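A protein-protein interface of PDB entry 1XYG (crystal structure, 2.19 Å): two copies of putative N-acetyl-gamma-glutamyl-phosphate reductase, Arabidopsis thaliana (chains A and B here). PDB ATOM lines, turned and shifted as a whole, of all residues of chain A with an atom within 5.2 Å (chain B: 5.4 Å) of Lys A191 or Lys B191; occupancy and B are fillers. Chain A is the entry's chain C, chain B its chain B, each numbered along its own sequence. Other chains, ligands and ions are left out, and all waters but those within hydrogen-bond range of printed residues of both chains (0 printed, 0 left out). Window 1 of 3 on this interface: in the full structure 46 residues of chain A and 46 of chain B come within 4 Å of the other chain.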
ATOM      1  N   TYR A 164      -3.800 -10.598  -4.637  1.00  0.00           N
ATOM      2  CA  TYR A 164      -4.876 -10.021  -3.833  1.00  0.00           C
ATOM      3  C   TYR A 164      -5.600  -8.874  -4.540  1.00  0.00           C
ATOM      4  O   TYR A 164      -6.831  -8.855  -4.610  1.00  0.00           O
ATOM      5  CB  TYR A 164      -4.333  -9.512  -2.492  1.00  0.00           C
ATOM      6  CG  TYR A 164      -4.039 -10.590  -1.476  1.00  0.00           C
ATOM      7  CD1 TYR A 164      -5.042 -11.448  -1.035  1.00  0.00           C
ATOM      8  CD2 TYR A 164      -2.770 -10.716  -0.918  1.00  0.00           C
ATOM      9  CE1 TYR A 164      -4.794 -12.401  -0.059  1.00  0.00           C
ATOM     10  CE2 TYR A 164      -2.505 -11.667   0.062  1.00  0.00           C
ATOM     11  CZ  TYR A 164      -3.523 -12.506   0.491  1.00  0.00           C
ATOM     12  OH  TYR A 164      -3.279 -13.428   1.488  1.00  0.00           O
ATOM     13  N   ASP A 189     -10.995  -8.862   4.193  1.00  0.00           N
ATOM     14  CA  ASP A 189     -10.338  -9.923   4.937  1.00  0.00           C
ATOM     15  C   ASP A 189      -9.993 -10.996   3.902  1.00  0.00           C
ATOM     16  O   ASP A 189     -10.863 -11.766   3.475  1.00  0.00           O
ATOM     17  CB  ASP A 189     -11.263 -10.494   6.015  1.00  0.00           C
ATOM     18  CG  ASP A 189     -10.534 -11.445   6.948  1.00  0.00           C
ATOM     19  OD1 ASP A 189     -10.071 -12.508   6.470  1.00  0.00           O
ATOM     20  OD2 ASP A 189     -10.407 -11.121   8.150  1.00  0.00           O
ATOM     21  N   ALA A 190      -8.723 -11.039   3.497  1.00  0.00           N
ATOM     22  CA  ALA A 190      -8.271 -11.982   2.481  1.00  0.00           C
ATOM     23  C   ALA A 190      -7.487 -13.190   2.988  1.00  0.00           C
ATOM     24  O   ALA A 190      -6.863 -13.163   4.057  1.00  0.00           O
ATOM     25  CB  ALA A 190      -7.464 -11.241   1.422  1.00  0.00           C
ATOM     26  N   LYS A 191      -7.529 -14.251   2.189  1.00  0.00           N
ATOM     27  CA  LYS A 191      -6.870 -15.505   2.513  1.00  0.00           C
ATOM     28  C   LYS A 191      -6.111 -16.002   1.295  1.00  0.00           C
ATOM     29  O   LYS A 191      -6.581 -15.869   0.162  1.00  0.00           O
ATOM     30  CB  LYS A 191      -7.907 -16.554   2.910  1.00  0.00           C
ATOM     31  CG  LYS A 191      -8.826 -16.180   4.083  1.00  0.00           C
ATOM     32  CD  LYS A 191      -9.961 -15.235   3.709  1.00  0.00           C
ATOM     33  CE  LYS A 191     -10.919 -15.083   4.898  1.00  0.00           C
ATOM     34  NZ  LYS A 191     -11.964 -14.018   4.744  1.00  0.00           N
ATOM     35  N   SER A 192      -4.948 -16.596   1.524  1.00  0.00           N
ATOM     36  CA  SER A 192      -4.154 -17.096   0.418  1.00  0.00           C
ATOM     37  C   SER A 192      -3.374 -18.351   0.740  1.00  0.00           C
ATOM     38  O   SER A 192      -2.945 -18.551   1.878  1.00  0.00           O
ATOM     39  CB  SER A 192      -3.180 -16.012  -0.059  1.00  0.00           C
ATOM     40  OG  SER A 192      -2.264 -16.533  -1.006  1.00  0.00           O
ATOM     41  N   GLY A 193      -3.199 -19.195  -0.277  1.00  0.00           N
ATOM     42  CA  GLY A 193      -2.421 -20.404  -0.116  1.00  0.00           C
ATOM     43  C   GLY A 193      -0.978 -19.953   0.044  1.00  0.00           C
ATOM     44  O   GLY A 193      -0.606 -18.871  -0.421  1.00  0.00           O
ATOM     45  N   ILE A 214      -3.711 -21.478  10.755  1.00  0.00           N
ATOM     46  CA  ILE A 214      -3.717 -20.255   9.962  1.00  0.00           C
ATOM     47  C   ILE A 214      -3.221 -19.105  10.829  1.00  0.00           C
ATOM     48  O   ILE A 214      -3.070 -19.250  12.052  1.00  0.00           O
ATOM     49  CB  ILE A 214      -5.133 -19.876   9.440  1.00  0.00           C
ATOM     50  CG1 ILE A 214      -6.077 -19.578  10.609  1.00  0.00           C
ATOM     51  CG2 ILE A 214      -5.673 -20.976   8.540  1.00  0.00           C
ATOM     52  CD1 ILE A 214      -7.337 -18.825  10.190  1.00  0.00           C
ATOM     53  N   HIS A 247      -4.266 -13.344   5.194  1.00  0.00           N
ATOM     54  CA  HIS A 247      -4.243 -14.495   6.087  1.00  0.00           C
ATOM     55  C   HIS A 247      -3.595 -15.636   5.326  1.00  0.00           C
ATOM     56  O   HIS A 247      -3.902 -15.859   4.154  1.00  0.00           O
ATOM     57  CB  HIS A 247      -5.658 -14.900   6.507  1.00  0.00           C
ATOM     58  CG  HIS A 247      -6.348 -13.893   7.371  1.00  0.00           C
ATOM     59  ND1 HIS A 247      -6.819 -12.692   6.886  1.00  0.00           N
ATOM     60  CD2 HIS A 247      -6.648 -13.911   8.691  1.00  0.00           C
ATOM     61  CE1 HIS A 247      -7.378 -12.011   7.870  1.00  0.00           C
ATOM     62  NE2 HIS A 247      -7.288 -12.727   8.977  1.00  0.00           N
ATOM     63  N   MET A 249      -3.130 -19.445   4.493  1.00  0.00           N
ATOM     64  CA  MET A 249      -3.859 -20.708   4.541  1.00  0.00           C
ATOM     65  C   MET A 249      -2.976 -21.947   4.396  1.00  0.00           C
ATOM     66  O   MET A 249      -2.014 -21.948   3.625  1.00  0.00           O
ATOM     67  CB  MET A 249      -4.910 -20.747   3.424  1.00  0.00           C
ATOM     68  CG  MET A 249      -5.923 -19.609   3.429  1.00  0.00           C
ATOM     69  SD  MET A 249      -7.018 -19.670   4.863  1.00  0.00           S
ATOM     70  CE  MET A 249      -6.188 -18.501   5.955  1.00  0.00           C
ATOM     71  N   GLY A 254      -4.826 -21.078  -4.192  1.00  0.00           N
ATOM     72  CA  GLY A 254      -6.119 -20.579  -3.783  1.00  0.00           C
ATOM     73  C   GLY A 254      -6.088 -19.253  -3.058  1.00  0.00           C
ATOM     74  O   GLY A 254      -5.209 -18.987  -2.230  1.00  0.00           O
ATOM     75  N   MET A 255      -7.066 -18.418  -3.370  1.00  0.00           N
ATOM     76  CA  MET A 255      -7.161 -17.116  -2.755  1.00  0.00           C
ATOM     77  C   MET A 255      -8.600 -16.640  -2.705  1.00  0.00           C
ATOM     78  O   MET A 255      -9.368 -16.810  -3.662  1.00  0.00           O
ATOM     79  CB  MET A 255      -6.310 -16.101  -3.529  1.00  0.00           C
ATOM     80  CG  MET A 255      -6.386 -14.676  -3.003  1.00  0.00           C
ATOM     81  SD  MET A 255      -5.201 -13.566  -3.816  1.00  0.00           S
ATOM     82  CE  MET A 255      -3.693 -14.085  -3.063  1.00  0.00           C
ATOM     83  N   GLN A 256      -8.961 -16.054  -1.573  1.00  0.00           N
ATOM     84  CA  GLN A 256     -10.287 -15.507  -1.406  1.00  0.00           C
ATOM     85  C   GLN A 256     -10.245 -14.191  -0.665  1.00  0.00           C
ATOM     86  O   GLN A 256      -9.512 -14.035   0.307  1.00  0.00           O
ATOM     87  CB  GLN A 256     -11.202 -16.454  -0.625  1.00  0.00           C
ATOM     88  CG  GLN A 256     -12.598 -15.845  -0.399  1.00  0.00           C
ATOM     89  CD  GLN A 256     -13.562 -16.766   0.328  1.00  0.00           C
ATOM     90  OE1 GLN A 256     -13.691 -17.941  -0.001  1.00  0.00           O
ATOM     91  NE2 GLN A 256     -14.254 -16.224   1.313  1.00  0.00           N
ATOM     92  N   SER A 257     -11.013 -13.234  -1.158  1.00  0.00           N
ATOM     93  CA  SER A 257     -11.146 -11.960  -0.481  1.00  0.00           C
ATOM     94  C   SER A 257     -12.615 -11.897  -0.075  1.00  0.00           C
ATOM     95  O   SER A 257     -13.500 -12.098  -0.907  1.00  0.00           O
ATOM     96  CB  SER A 257     -10.833 -10.773  -1.400  1.00  0.00           C
ATOM     97  OG  SER A 257      -9.442 -10.522  -1.468  1.00  0.00           O
ATOM     98  N   THR A 258     -12.861 -11.691   1.211  1.00  0.00           N
ATOM     99  CA  THR A 258     -14.220 -11.536   1.710  1.00  0.00           C
ATOM    100  C   THR A 258     -14.267 -10.025   1.930  1.00  0.00           C
ATOM    101  O   THR A 258     -13.588  -9.493   2.807  1.00  0.00           O
ATOM    102  CB  THR A 258     -14.448 -12.289   3.032  1.00  0.00           C
ATOM    103  OG1 THR A 258     -14.216 -13.692   2.833  1.00  0.00           O
ATOM    104  CG2 THR A 258     -15.893 -12.087   3.505  1.00  0.00           C
ATOM    105  N   TYR B 164     -17.017 -20.355  18.080  1.00  0.00           N
ATOM    106  CA  TYR B 164     -16.855 -19.000  17.563  1.00  0.00           C
ATOM    107  C   TYR B 164     -17.175 -17.932  18.616  1.00  0.00           C
ATOM    108  O   TYR B 164     -16.375 -17.019  18.841  1.00  0.00           O
ATOM    109  CB  TYR B 164     -17.739 -18.783  16.332  1.00  0.00           C
ATOM    110  CG  TYR B 164     -17.214 -19.389  15.044  1.00  0.00           C
ATOM    111  CD1 TYR B 164     -16.009 -18.961  14.489  1.00  0.00           C
ATOM    112  CD2 TYR B 164     -17.958 -20.344  14.346  1.00  0.00           C
ATOM    113  CE1 TYR B 164     -15.555 -19.459  13.265  1.00  0.00           C
ATOM    114  CE2 TYR B 164     -17.514 -20.854  13.115  1.00  0.00           C
ATOM    115  CZ  TYR B 164     -16.311 -20.402  12.580  1.00  0.00           C
ATOM    116  OH  TYR B 164     -15.870 -20.877  11.356  1.00  0.00           O
ATOM    117  N   ASP B 189     -14.794 -11.696  10.820  1.00  0.00           N
ATOM    118  CA  ASP B 189     -14.480 -12.639   9.760  1.00  0.00           C
ATOM    119  C   ASP B 189     -13.772 -13.799  10.455  1.00  0.00           C
ATOM    120  O   ASP B 189     -12.594 -13.703  10.794  1.00  0.00           O
ATOM    121  CB  ASP B 189     -13.564 -11.986   8.724  1.00  0.00           C
ATOM    122  CG  ASP B 189     -13.304 -12.881   7.539  1.00  0.00           C
ATOM    123  OD1 ASP B 189     -12.735 -13.975   7.747  1.00  0.00           O
ATOM    124  OD2 ASP B 189     -13.676 -12.493   6.410  1.00  0.00           O
ATOM    125  N   ALA B 190     -14.495 -14.893  10.678  1.00  0.00           N
ATOM    126  CA  ALA B 190     -13.936 -16.039  11.382  1.00  0.00           C
ATOM    127  C   ALA B 190     -13.570 -17.242  10.519  1.00  0.00           C
ATOM    128  O   ALA B 190     -14.106 -17.449   9.424  1.00  0.00           O
ATOM    129  CB  ALA B 190     -14.884 -16.462  12.495  1.00  0.00           C
ATOM    130  N   LYS B 191     -12.643 -18.039  11.039  1.00  0.00           N
ATOM    131  CA  LYS B 191     -12.156 -19.226  10.354  1.00  0.00           C
ATOM    132  C   LYS B 191     -12.118 -20.396  11.317  1.00  0.00           C
ATOM    133  O   LYS B 191     -11.785 -20.243  12.495  1.00  0.00           O
ATOM    134  CB  LYS B 191     -10.743 -18.982   9.822  1.00  0.00           C
ATOM    135  CG  LYS B 191     -10.622 -17.812   8.865  1.00  0.00           C
ATOM    136  CD  LYS B 191     -10.516 -16.476   9.568  1.00  0.00           C
ATOM    137  CE  LYS B 191     -10.161 -15.397   8.556  1.00  0.00           C
ATOM    138  NZ  LYS B 191     -10.261 -14.016   9.073  1.00  0.00           N
ATOM    139  N   SER B 192     -12.430 -21.579  10.817  1.00  0.00           N
ATOM    140  CA  SER B 192     -12.414 -22.751  11.668  1.00  0.00           C
ATOM    141  C   SER B 192     -11.993 -24.018  10.951  1.00  0.00           C
ATOM    142  O   SER B 192     -12.249 -24.183   9.760  1.00  0.00           O
ATOM    143  CB  SER B 192     -13.794 -22.981  12.277  1.00  0.00           C
ATOM    144  OG  SER B 192     -13.787 -24.188  13.015  1.00  0.00           O
ATOM    145  N   GLY B 193     -11.342 -24.909  11.692  1.00  0.00           N
ATOM    146  CA  GLY B 193     -10.939 -26.184  11.138  1.00  0.00           C
ATOM    147  C   GLY B 193     -12.223 -26.975  10.949  1.00  0.00           C
ATOM    148  O   GLY B 193     -13.221 -26.725  11.638  1.00  0.00           O
ATOM    149  N   ILE B 214     -10.595 -23.195   0.567  1.00  0.00           N
ATOM    150  CA  ILE B 214     -11.421 -22.650   1.630  1.00  0.00           C
ATOM    151  C   ILE B 214     -12.714 -22.128   1.025  1.00  0.00           C
ATOM    152  O   ILE B 214     -12.844 -22.014  -0.198  1.00  0.00           O
ATOM    153  CB  ILE B 214     -10.749 -21.461   2.355  1.00  0.00           C
ATOM    154  CG1 ILE B 214     -10.593 -20.290   1.385  1.00  0.00           C
ATOM    155  CG2 ILE B 214      -9.411 -21.874   2.923  1.00  0.00           C
ATOM    156  CD1 ILE B 214     -10.289 -18.991   2.077  1.00  0.00           C
ATOM    157  N   THR B 245     -19.126 -13.709   9.662  1.00  0.00           N
ATOM    158  CA  THR B 245     -18.989 -14.617   8.533  1.00  0.00           C
ATOM    159  C   THR B 245     -17.973 -15.732   8.778  1.00  0.00           C
ATOM    160  O   THR B 245     -16.774 -15.488   8.852  1.00  0.00           O
ATOM    161  CB  THR B 245     -18.579 -13.857   7.235  1.00  0.00           C
ATOM    162  OG1 THR B 245     -19.403 -12.697   7.067  1.00  0.00           O
ATOM    163  CG2 THR B 245     -18.761 -14.749   6.001  1.00  0.00           C
ATOM    164  N   PRO B 246     -18.453 -16.978   8.926  1.00  0.00           N
ATOM    165  CA  PRO B 246     -17.595 -18.148   9.154  1.00  0.00           C
ATOM    166  C   PRO B 246     -16.909 -18.565   7.854  1.00  0.00           C
ATOM    167  O   PRO B 246     -17.405 -18.281   6.760  1.00  0.00           O
ATOM    168  CB  PRO B 246     -18.579 -19.224   9.610  1.00  0.00           C
ATOM    169  CG  PRO B 246     -19.736 -18.459  10.135  1.00  0.00           C
ATOM    170  CD  PRO B 246     -19.864 -17.320   9.166  1.00  0.00           C
ATOM    171  N   HIS B 247     -15.774 -19.245   7.983  1.00  0.00           N
ATOM    172  CA  HIS B 247     -15.017 -19.741   6.835  1.00  0.00           C
ATOM    173  C   HIS B 247     -14.467 -21.108   7.224  1.00  0.00           C
ATOM    174  O   HIS B 247     -13.976 -21.290   8.341  1.00  0.00           O
ATOM    175  CB  HIS B 247     -13.863 -18.791   6.469  1.00  0.00           C
ATOM    176  CG  HIS B 247     -14.313 -17.468   5.922  1.00  0.00           C
ATOM    177  ND1 HIS B 247     -14.858 -16.480   6.713  1.00  0.00           N
ATOM    178  CD2 HIS B 247     -14.326 -16.984   4.657  1.00  0.00           C
ATOM    179  CE1 HIS B 247     -15.191 -15.447   5.961  1.00  0.00           C
ATOM    180  NE2 HIS B 247     -14.880 -15.726   4.707  1.00  0.00           N
ATOM    181  N   MET B 249     -11.770 -23.958   7.041  1.00  0.00           N
ATOM    182  CA  MET B 249     -10.345 -24.139   6.766  1.00  0.00           C
ATOM    183  C   MET B 249      -9.947 -25.586   6.506  1.00  0.00           C
ATOM    184  O   MET B 249     -10.481 -26.505   7.125  1.00  0.00           O
ATOM    185  CB  MET B 249      -9.513 -23.637   7.948  1.00  0.00           C
ATOM    186  CG  MET B 249      -9.724 -22.184   8.318  1.00  0.00           C
ATOM    187  SD  MET B 249      -9.140 -21.027   7.060  1.00  0.00           S
ATOM    188  CE  MET B 249     -10.724 -20.517   6.273  1.00  0.00           C
ATOM    189  N   GLY B 254      -8.425 -25.753  15.200  1.00  0.00           N
ATOM    190  CA  GLY B 254      -8.028 -24.366  15.073  1.00  0.00           C
ATOM    191  C   GLY B 254      -9.146 -23.419  14.709  1.00  0.00           C
ATOM    192  O   GLY B 254     -10.024 -23.727  13.894  1.00  0.00           O
ATOM    193  N   MET B 255      -9.102 -22.240  15.309  1.00  0.00           N
ATOM    194  CA  MET B 255     -10.120 -21.247  15.055  1.00  0.00           C
ATOM    195  C   MET B 255      -9.574 -19.854  15.289  1.00  0.00           C
ATOM    196  O   MET B 255      -8.835 -19.612  16.250  1.00  0.00           O
ATOM    197  CB  MET B 255     -11.334 -21.488  15.967  1.00  0.00           C
ATOM    198  CG  MET B 255     -12.414 -20.414  15.881  1.00  0.00           C
ATOM    199  SD  MET B 255     -13.926 -20.859  16.782  1.00  0.00           S
ATOM    200  CE  MET B 255     -14.688 -21.993  15.659  1.00  0.00           C
ATOM    201  N   GLN B 256      -9.939 -18.945  14.398  1.00  0.00           N
ATOM    202  CA  GLN B 256      -9.521 -17.569  14.519  1.00  0.00           C
ATOM    203  C   GLN B 256     -10.630 -16.628  14.115  1.00  0.00           C
ATOM    204  O   GLN B 256     -11.328 -16.850  13.128  1.00  0.00           O
ATOM    205  CB  GLN B 256      -8.299 -17.251  13.643  1.00  0.00           C
ATOM    206  CG  GLN B 256      -7.992 -15.742  13.640  1.00  0.00           C
ATOM    207  CD  GLN B 256      -6.676 -15.371  12.966  1.00  0.00           C
ATOM    208  OE1 GLN B 256      -5.683 -16.090  13.062  1.00  0.00           O
ATOM    209  NE2 GLN B 256      -6.661 -14.228  12.308  1.00  0.00           N
ATOM    210  N   SER B 257     -10.800 -15.576  14.900  1.00  0.00           N
ATOM    211  CA  SER B 257     -11.767 -14.561  14.566  1.00  0.00           C
ATOM    212  C   SER B 257     -10.936 -13.309  14.364  1.00  0.00           C
ATOM    213  O   SER B 257     -10.118 -12.958  15.209  1.00  0.00           O
ATOM    214  CB  SER B 257     -12.781 -14.344  15.697  1.00  0.00           C
ATOM    215  OG  SER B 257     -13.803 -15.330  15.667  1.00  0.00           O
ATOM    216  N   THR B 258     -11.106 -12.676  13.214  1.00  0.00           N
ATOM    217  CA  THR B 258     -10.416 -11.432  12.934  1.00  0.00           C
ATOM    218  C   THR B 258     -11.555 -10.436  13.098  1.00  0.00           C
ATOM    219  O   THR B 258     -12.499 -10.410  12.303  1.00  0.00           O
ATOM    220  CB  THR B 258      -9.845 -11.404  11.511  1.00  0.00           C
ATOM    221  OG1 THR B 258      -8.948 -12.516  11.349  1.00  0.00           O
ATOM    222  CG2 THR B 258      -9.085 -10.094  11.268  1.00  0.00           C
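The side-chain carboxylate (OD1) of Asp A189 lies close to the side-chain carboxylate (OD1) of Asp B189, 3.3 Å away. The side-chain hydroxyl of Thr B258 is in hydrogen-bond range of a ring nitrogen (NE2) of His A247, at 2.9 Å. A ring nitrogen (NE2) of His B247 lies within hydrogen-bond range of the side-chain hydroxyl of Thr A258. The side-chain carboxylate (OD2) of Asp B189 is in salt-bridge range of the side-chain amino group (NZ) of Lys A191. A ring nitrogen (NE2) of His B247 is in hydrogen-bond range of the side-chain amino group (NZ) of Lys A191. The side-chain sulfur of Met B249 lies close to the side-chain sulfur of Met A249, 3.3 Å away. A ring nitrogen (NE2) of His A247 is in hydrogen-bond range of the side-chain amino group (NZ) of Lys B191, at 3.2 Å. The side-chain amino group (NZ) of Lys B191 is in salt-bridge range of the side-chain carboxylate (OD1) of Asp A189, at 3.0 Å. A ring nitrogen (NE2) of His B247 lies close to the side-chain amide nitrogen of Gln A256 (3.5 Å).
N of Lys B191 lies within hydrogen-bond range of O of Gln B256. The backbone NH (N) of Ser B192 sits at hydrogen-bond distance from the backbone carbonyl oxygen (O) of His B247 (2.9 Å). A ring nitrogen (ND1) of His B247 sits at hydrogen-bond distance from the backbone carbonyl oxygen (O) of Thr B245, at 3.0 Å. O of Ala B190 lies within hydrogen-bond range of N of His B247. The backbone carbonyl oxygen of Ser B192 sits at hydrogen-bond distance from the backbone NH of Met B249, 2.8 Å away. ND1 of His B247 lies close to OD1 of Asp B189 (3.4 Å).
Of the printed residues of chain B, Asp A189 touches Asp B189 (3.2 Å), Lys B191 (3.0 Å) and Thr B258 (3.4 Å). Lys A191 touches four residues of chain B. Of chain A, only Asp A189 (3.0 Å), Lys A191 (3.7 Å), Ile A214 (3.4 Å) and His A247 (3.2 Å) come within 4 Å of Lys B191. Of the printed residues of chain A, Ile B214 touches Lys A191 (3.5 Å), Met A249 (3.8 Å) and Gln A256 (3.8 Å). Of the printed residues of chain A, His B247 touches Lys A191 (3.4 Å), Gln A256 (3.4 Å) and Thr A258 (2.8 Å).
Asp A189 touches its own counterpart, Asp B189. Lys A191 touches His B247, and with the chains exchanged His A247 touches Lys B191. Ile A214 touches Gln B256, and with the chains exchanged Gln A256 touches Ile B214. His A247 touches Thr B258, and with the chains exchanged Thr A258 touches His B247. 14 positions are printed for both chains. Of the 19 pairs that touch across the chains among the printed residues, 19 have their exchanged pair printed and touching as well.
Hydrophobic or aromatic side chains of chain B within 4 Å of the printed part of chain A: Ile B214, His B247 and Met B249. Of the 14 printed residues of chain A, 7 touch a printed residue of chain B. Printed residues of chain A that touch a printed residue of chain B: Asp A189, Lys A191, Ile A214, His A247, Met A249, Gln A256 and Thr A258. Hydrophobic or aromatic side chains of chain A within 4 Å of the printed part of chain B: Ile A214, His A247 and Met A249. Among the printed residues, 19 pairs touch across the chains. Among the printed residues, Asp or Glu carboxylates within 4 Å of a Lys or Arg side-chain nitrogen of the other chain: Asp A189 with Lys B191 (3.0 Å) and Lys A191 with Asp B189 (2.8 Å).
Among the printed residues, pairs that only touch across the chains: Asp A189 with Thr B258 (3.4 Å), Lys A191 with Lys B191 (3.7 Å), Lys A191 with Ile B214 (3.5 Å), Ile A214 with Lys B191 (3.4 Å), Ile A214 with Met B249 (3.8 Å), Ile A214 with Gln B256 (3.9 Å), His A247 with Gln B256 (3.6 Å), Met A249 with Ile B214 (3.8 Å), Gln A256 with Ile B214 (3.8 Å) and Thr A258 with Asp B189 (3.5 Å).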
